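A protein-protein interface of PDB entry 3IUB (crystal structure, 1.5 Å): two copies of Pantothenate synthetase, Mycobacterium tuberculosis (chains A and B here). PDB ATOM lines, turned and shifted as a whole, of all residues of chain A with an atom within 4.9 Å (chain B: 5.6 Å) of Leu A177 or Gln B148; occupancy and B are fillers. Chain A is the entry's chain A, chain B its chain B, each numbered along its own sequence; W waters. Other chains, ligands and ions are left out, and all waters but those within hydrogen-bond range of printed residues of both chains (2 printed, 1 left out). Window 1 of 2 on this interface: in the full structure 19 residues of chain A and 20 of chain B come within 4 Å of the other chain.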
ATOM      1  N   LEU A 144     -23.675 -18.016  30.873  1.00  0.00           N
ATOM      2  CA  LEU A 144     -23.245 -19.391  31.097  1.00  0.00           C
ATOM      3  C   LEU A 144     -22.867 -19.597  32.565  1.00  0.00           C
ATOM      4  O   LEU A 144     -23.295 -20.573  33.174  1.00  0.00           O
ATOM      5  CB  LEU A 144     -22.090 -19.774  30.146  1.00  0.00           C
ATOM      6  CG  LEU A 144     -21.546 -21.215  30.288  1.00  0.00           C
ATOM      7  CD1 LEU A 144     -22.672 -22.262  30.102  1.00  0.00           C
ATOM      8  CD2 LEU A 144     -20.402 -21.500  29.330  1.00  0.00           C
ATOM      9  N   LEU A 147     -25.969 -19.623  34.847  1.00  0.00           N
ATOM     10  CA  LEU A 147     -26.703 -20.866  34.643  1.00  0.00           C
ATOM     11  C   LEU A 147     -26.037 -22.018  35.379  1.00  0.00           C
ATOM     12  O   LEU A 147     -26.720 -22.894  35.902  1.00  0.00           O
ATOM     13  CB  LEU A 147     -26.813 -21.205  33.161  1.00  0.00           C
ATOM     14  CG  LEU A 147     -27.786 -20.308  32.413  1.00  0.00           C
ATOM     15  CD1 LEU A 147     -27.662 -20.603  30.932  1.00  0.00           C
ATOM     16  CD2 LEU A 147     -29.198 -20.554  32.851  1.00  0.00           C
ATOM     17  N   GLN A 148     -24.706 -22.021  35.410  1.00  0.00           N
ATOM     18  CA  GLN A 148     -23.964 -23.101  36.066  1.00  0.00           C
ATOM     19  C   GLN A 148     -24.001 -22.935  37.566  1.00  0.00           C
ATOM     20  O   GLN A 148     -24.050 -23.920  38.284  1.00  0.00           O
ATOM     21  CB  GLN A 148     -22.516 -23.175  35.562  1.00  0.00           C
ATOM     22  CG  GLN A 148     -22.414 -23.534  34.075  1.00  0.00           C
ATOM     23  CD  GLN A 148     -22.926 -24.931  33.744  1.00  0.00           C
ATOM     24  OE1 GLN A 148     -22.828 -25.843  34.543  1.00  0.00           O
ATOM     25  NE2 GLN A 148     -23.427 -25.102  32.525  1.00  0.00           N
ATOM     26  N   LEU A 171     -26.574 -20.471  22.631  1.00  0.00           N
ATOM     27  CA  LEU A 171     -25.728 -20.954  23.725  1.00  0.00           C
ATOM     28  C   LEU A 171     -26.295 -22.238  24.332  1.00  0.00           C
ATOM     29  O   LEU A 171     -25.578 -23.251  24.481  1.00  0.00           O
ATOM     30  CB  LEU A 171     -25.653 -19.862  24.796  1.00  0.00           C
ATOM     31  CG  LEU A 171     -24.940 -20.256  26.084  1.00  0.00           C
ATOM     32  CD1 LEU A 171     -23.442 -20.237  25.907  1.00  0.00           C
ATOM     33  CD2 LEU A 171     -25.305 -19.293  27.195  1.00  0.00           C
ATOM     34  N   VAL A 172     -27.573 -22.196  24.687  1.00  0.00           N
ATOM     35  CA  VAL A 172     -28.244 -23.345  25.288  1.00  0.00           C
ATOM     36  C   VAL A 172     -28.245 -24.606  24.402  1.00  0.00           C
ATOM     37  O   VAL A 172     -27.929 -25.708  24.883  1.00  0.00           O
ATOM     38  CB  VAL A 172     -29.645 -22.941  25.810  1.00  0.00           C
ATOM     39  CG1 VAL A 172     -30.480 -24.182  26.190  1.00  0.00           C
ATOM     40  CG2 VAL A 172     -29.494 -21.952  26.996  1.00  0.00           C
ATOM     41  N   PHE A 175     -24.303 -25.783  23.615  1.00  0.00           N
ATOM     42  CA  PHE A 175     -23.596 -26.381  24.737  1.00  0.00           C
ATOM     43  C   PHE A 175     -24.449 -27.440  25.459  1.00  0.00           C
ATOM     44  O   PHE A 175     -24.048 -27.955  26.513  1.00  0.00           O
ATOM     45  CB  PHE A 175     -23.111 -25.319  25.719  1.00  0.00           C
ATOM     46  CG  PHE A 175     -21.998 -24.457  25.191  1.00  0.00           C
ATOM     47  CD1 PHE A 175     -21.270 -24.816  24.069  1.00  0.00           C
ATOM     48  CD2 PHE A 175     -21.653 -23.302  25.845  1.00  0.00           C
ATOM     49  CE1 PHE A 175     -20.217 -24.014  23.603  1.00  0.00           C
ATOM     50  CE2 PHE A 175     -20.593 -22.486  25.392  1.00  0.00           C
ATOM     51  CZ  PHE A 175     -19.874 -22.855  24.261  1.00  0.00           C
ATOM     52  N   ASN A 176     -25.591 -27.824  24.885  1.00  0.00           N
ATOM     53  CA  ASN A 176     -26.406 -28.895  25.478  1.00  0.00           C
ATOM     54  C   ASN A 176     -26.828 -28.585  26.913  1.00  0.00           C
ATOM     55  O   ASN A 176     -26.923 -29.490  27.733  1.00  0.00           O
ATOM     56  CB  ASN A 176     -25.657 -30.230  25.432  1.00  0.00           C
ATOM     57  CG  ASN A 176     -25.241 -30.613  24.023  1.00  0.00           C
ATOM     58  OD1 ASN A 176     -24.121 -30.327  23.594  1.00  0.00           O
ATOM     59  ND2 ASN A 176     -26.149 -31.254  23.289  1.00  0.00           N
ATOM     60  N   LEU A 177     -27.113 -27.315  27.198  1.00  0.00           N
ATOM     61  CA  LEU A 177     -27.504 -26.914  28.574  1.00  0.00           C
ATOM     62  C   LEU A 177     -28.904 -27.403  28.935  1.00  0.00           C
ATOM     63  O   LEU A 177     -29.817 -27.335  28.113  1.00  0.00           O
ATOM     64  CB  LEU A 177     -27.374 -25.393  28.783  1.00  0.00           C
ATOM     65  CG  LEU A 177     -26.038 -24.731  28.383  1.00  0.00           C
ATOM     66  CD1 LEU A 177     -26.042 -23.232  28.627  1.00  0.00           C
ATOM     67  CD2 LEU A 177     -24.824 -25.348  29.060  1.00  0.00           C
ATOM     68  N   ASP A 178     -29.059 -27.905  30.163  1.00  0.00           N
ATOM     69  CA  ASP A 178     -30.324 -28.515  30.585  1.00  0.00           C
ATOM     70  C   ASP A 178     -31.174 -27.453  31.259  1.00  0.00           C
ATOM     71  O   ASP A 178     -31.415 -27.500  32.473  1.00  0.00           O
ATOM     72  CB  ASP A 178     -30.069 -29.697  31.541  1.00  0.00           C
ATOM     73  CG  ASP A 178     -31.327 -30.542  31.794  1.00  0.00           C
ATOM     74  OD1 ASP A 178     -32.342 -30.378  31.078  1.00  0.00           O
ATOM     75  OD2 ASP A 178     -31.295 -31.384  32.718  1.00  0.00           O
ATOM     76  N   VAL A 179     -31.567 -26.454  30.478  1.00  0.00           N
ATOM     77  CA  VAL A 179     -32.420 -25.364  30.963  1.00  0.00           C
ATOM     78  C   VAL A 179     -33.344 -24.987  29.832  1.00  0.00           C
ATOM     79  O   VAL A 179     -32.941 -25.036  28.662  1.00  0.00           O
ATOM     80  CB  VAL A 179     -31.589 -24.115  31.399  1.00  0.00           C
ATOM     81  CG1 VAL A 179     -30.774 -23.517  30.217  1.00  0.00           C
ATOM     82  CG2 VAL A 179     -32.473 -23.055  32.003  1.00  0.00           C
ATOM     83  N   VAL B 143     -15.571 -31.096  25.410  1.00  0.00           N
ATOM     84  CA  VAL B 143     -15.614 -31.497  26.818  1.00  0.00           C
ATOM     85  C   VAL B 143     -16.770 -30.802  27.541  1.00  0.00           C
ATOM     86  O   VAL B 143     -17.514 -31.439  28.299  1.00  0.00           O
ATOM     87  CB  VAL B 143     -14.284 -31.274  27.533  1.00  0.00           C
ATOM     88  CG1 VAL B 143     -14.461 -31.465  29.036  1.00  0.00           C
ATOM     89  CG2 VAL B 143     -13.242 -32.268  26.987  1.00  0.00           C
ATOM     90  N   LEU B 144     -16.950 -29.517  27.263  1.00  0.00           N
ATOM     91  CA  LEU B 144     -18.075 -28.810  27.848  1.00  0.00           C
ATOM     92  C   LEU B 144     -19.406 -29.480  27.503  1.00  0.00           C
ATOM     93  O   LEU B 144     -20.242 -29.712  28.370  1.00  0.00           O
ATOM     94  CB  LEU B 144     -18.083 -27.348  27.406  1.00  0.00           C
ATOM     95  CG  LEU B 144     -19.218 -26.512  28.024  1.00  0.00           C
ATOM     96  CD1 LEU B 144     -19.232 -26.495  29.585  1.00  0.00           C
ATOM     97  CD2 LEU B 144     -19.133 -25.092  27.454  1.00  0.00           C
ATOM     98  N   LYS B 145     -19.588 -29.781  26.224  1.00  0.00           N
ATOM     99  CA  LYS B 145     -20.807 -30.434  25.755  1.00  0.00           C
ATOM    100  C   LYS B 145     -21.017 -31.787  26.426  1.00  0.00           C
ATOM    101  O   LYS B 145     -22.095 -32.077  26.874  1.00  0.00           O
ATOM    102  CB  LYS B 145     -20.776 -30.569  24.221  1.00  0.00           C
ATOM    103  CG  LYS B 145     -20.916 -29.194  23.531  1.00  0.00           C
ATOM    104  CD  LYS B 145     -20.576 -29.205  22.042  1.00  0.00           C
ATOM    105  CE  LYS B 145     -21.497 -30.159  21.254  1.00  0.00           C
ATOM    106  NZ  LYS B 145     -22.938 -29.779  21.248  1.00  0.00           N
ATOM    107  N   LEU B 146     -19.964 -32.608  26.498  1.00  0.00           N
ATOM    108  CA  LEU B 146     -20.112 -33.932  27.137  1.00  0.00           C
ATOM    109  C   LEU B 146     -20.501 -33.780  28.604  1.00  0.00           C
ATOM    110  O   LEU B 146     -21.345 -34.517  29.120  1.00  0.00           O
ATOM    111  CB  LEU B 146     -18.815 -34.733  27.013  1.00  0.00           C
ATOM    112  CG  LEU B 146     -18.437 -35.144  25.594  1.00  0.00           C
ATOM    113  CD1 LEU B 146     -17.022 -35.705  25.596  1.00  0.00           C
ATOM    114  CD2 LEU B 146     -19.415 -36.166  25.070  1.00  0.00           C
ATOM    115  N   LEU B 147     -19.894 -32.796  29.255  1.00  0.00           N
ATOM    116  CA  LEU B 147     -20.216 -32.525  30.651  1.00  0.00           C
ATOM    117  C   LEU B 147     -21.664 -32.124  30.833  1.00  0.00           C
ATOM    118  O   LEU B 147     -22.292 -32.496  31.822  1.00  0.00           O
ATOM    119  CB  LEU B 147     -19.320 -31.436  31.220  1.00  0.00           C
ATOM    120  CG  LEU B 147     -17.895 -31.926  31.464  1.00  0.00           C
ATOM    121  CD1 LEU B 147     -17.043 -30.728  31.829  1.00  0.00           C
ATOM    122  CD2 LEU B 147     -17.810 -33.001  32.538  1.00  0.00           C
ATOM    123  N   GLN B 148     -22.207 -31.376  29.883  1.00  0.00           N
ATOM    124  CA  GLN B 148     -23.602 -30.950  29.992  1.00  0.00           C
ATOM    125  C   GLN B 148     -24.562 -32.062  29.657  1.00  0.00           C
ATOM    126  O   GLN B 148     -25.634 -32.164  30.251  1.00  0.00           O
ATOM    127  CB  GLN B 148     -23.875 -29.737  29.091  1.00  0.00           C
ATOM    128  CG  GLN B 148     -23.006 -28.527  29.429  1.00  0.00           C
ATOM    129  CD  GLN B 148     -23.147 -28.079  30.885  1.00  0.00           C
ATOM    130  OE1 GLN B 148     -24.245 -27.984  31.413  1.00  0.00           O
ATOM    131  NE2 GLN B 148     -22.022 -27.817  31.535  1.00  0.00           N
ATOM    132  N   ILE B 149     -24.193 -32.895  28.691  1.00  0.00           N
ATOM    133  CA  ILE B 149     -25.048 -34.010  28.287  1.00  0.00           C
ATOM    134  C   ILE B 149     -25.146 -35.042  29.403  1.00  0.00           C
ATOM    135  O   ILE B 149     -26.231 -35.522  29.760  1.00  0.00           O
ATOM    136  CB  ILE B 149     -24.514 -34.709  27.022  1.00  0.00           C
ATOM    137  CG1 ILE B 149     -24.700 -33.792  25.810  1.00  0.00           C
ATOM    138  CG2 ILE B 149     -25.305 -36.009  26.785  1.00  0.00           C
ATOM    139  CD1 ILE B 149     -23.767 -34.112  24.632  1.00  0.00           C
ATOM    140  N   VAL B 150     -23.986 -35.421  29.924  1.00  0.00           N
ATOM    141  CA  VAL B 150     -23.894 -36.496  30.919  1.00  0.00           C
ATOM    142  C   VAL B 150     -24.105 -36.044  32.371  1.00  0.00           C
ATOM    143  O   VAL B 150     -24.630 -36.810  33.189  1.00  0.00           O
ATOM    144  CB  VAL B 150     -22.541 -37.237  30.746  1.00  0.00           C
ATOM    145  CG1 VAL B 150     -22.359 -38.366  31.792  1.00  0.00           C
ATOM    146  CG2 VAL B 150     -22.460 -37.845  29.312  1.00  0.00           C
ATOM    147  N   ARG B 151     -23.702 -34.808  32.668  1.00  0.00           N
ATOM    148  CA  ARG B 151     -23.781 -34.253  34.030  1.00  0.00           C
ATOM    149  C   ARG B 151     -23.186 -35.232  35.054  1.00  0.00           C
ATOM    150  O   ARG B 151     -23.859 -35.666  36.005  1.00  0.00           O
ATOM    151  CB  ARG B 151     -25.208 -33.845  34.408  1.00  0.00           C
ATOM    152  CG  ARG B 151     -25.262 -32.905  35.614  1.00  0.00           C
ATOM    153  CD  ARG B 151     -26.665 -32.847  36.210  1.00  0.00           C
ATOM    154  NE  ARG B 151     -26.846 -31.852  37.274  1.00  0.00           N
ATOM    155  CZ  ARG B 151     -26.405 -31.958  38.528  1.00  0.00           C
ATOM    156  NH1 ARG B 151     -25.695 -33.005  38.926  1.00  0.00           N
ATOM    157  NH2 ARG B 151     -26.661 -30.986  39.397  1.00  0.00           N
ATOM    158  N   PRO B 152     -21.903 -35.584  34.867  1.00  0.00           N
ATOM    159  CA  PRO B 152     -21.277 -36.511  35.786  1.00  0.00           C
ATOM    160  C   PRO B 152     -20.902 -35.836  37.084  1.00  0.00           C
ATOM    161  O   PRO B 152     -20.739 -34.601  37.137  1.00  0.00           O
ATOM    162  CB  PRO B 152     -19.996 -36.911  35.044  1.00  0.00           C
ATOM    163  CG  PRO B 152     -19.633 -35.690  34.228  1.00  0.00           C
ATOM    164  CD  PRO B 152     -20.960 -35.109  33.825  1.00  0.00           C
ATOM    165  N   LEU B 177     -18.431 -24.772  36.656  1.00  0.00           N
ATOM    166  CA  LEU B 177     -19.004 -26.137  36.510  1.00  0.00           C
ATOM    167  C   LEU B 177     -18.937 -26.940  37.811  1.00  0.00           C
ATOM    168  O   LEU B 177     -17.976 -26.838  38.551  1.00  0.00           O
ATOM    169  CB  LEU B 177     -18.336 -26.911  35.365  1.00  0.00           C
ATOM    170  CG  LEU B 177     -18.175 -26.180  34.017  1.00  0.00           C
ATOM    171  CD1 LEU B 177     -17.536 -27.124  32.991  1.00  0.00           C
ATOM    172  CD2 LEU B 177     -19.452 -25.651  33.457  1.00  0.00           C
HETATM  173  O   HOH W   1     -26.712 -29.275  31.442  1.00  0.00           O
HETATM  174  O   HOH W   2     -28.223 -31.608  28.727  1.00  0.00           O
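NE2 of Gln A148 lies within hydrogen-bond range of OE1 of Gln B148. NZ of Lys B145 sits at hydrogen-bond distance from OD1 of Asn A176 (2.7 Å).
The backbone carbonyl oxygen (O) of Val A172 lies within hydrogen-bond range of the backbone NH (N) of Leu A177 (2.9 Å).
Gln A148 touches Leu B177 (OE1 to CD2, 3.6 Å). Phe A175 touches Leu B144 (CD2 to CD2, 3.5 Å). Phe A175 touches Gln B148. Asn A176 touches Gln B148. Asn A176 touches Ile B149. Leu A177 touches Gln B148.
Printed residues of chain B within 4 Å of Gln A148: Gln B148 and Leu B177. Of the printed residues of chain B, Asn A176 touches Lys B145, Gln B148 and Ile B149. Printed residues of chain B within 4 Å of Leu A177: Gln B148 (3.6 Å). Of the printed residues of chain A, Leu B144 touches Phe A175. Gln B148 touches four residues of chain A. Printed residues of chain A within 4 Å of Leu B177: Gln A148 (3.6 Å). The nearest printed residue of chain B that does not touch Leu A177 is Leu B144 (5.7 Å). The nearest printed residue of chain A that does not touch Lys B145 is Phe A175 (4.1 Å).
Of the 11 printed residues of chain B, 5 touch a printed residue of chain A. Hydrophobic or aromatic side chains of chain B within 4 Å of the printed part of chain A: Leu B144, Ile B149 and Leu B177. Of the 10 printed residues of chain A, 4 touch a printed residue of chain B. Hydrophobic or aromatic side chains of chain A that line the printed part of chain B: Phe A175 and Leu A177. Among the printed residues, 8 pairs touch across the chains. Among the printed residues, no Asp or Glu carboxylate lies within 4 Å of a Lys or Arg side-chain nitrogen of the other chain.
Gln A148 touches its own counterpart, Gln B148. Gln A148 touches Leu B177, and with the chains exchanged Leu A177 touches Gln B148. Positions printed for both chains: 144, 147, 148 and 177. Of the 8 pairs that touch across the chains among the printed residues, 3 have their exchanged pair printed and touching as well.
Water W2 lies within hydrogen-bond range of the backbone carbonyl oxygen of Asn A176 (2.7 Å) and the backbone carbonyl oxygen of Gln B148 (3.1 Å). Water W1 bridges the side-chain amide oxygen of Gln B148 (2.8 Å) and the backbone NH of Asp A178 (3.0 Å).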
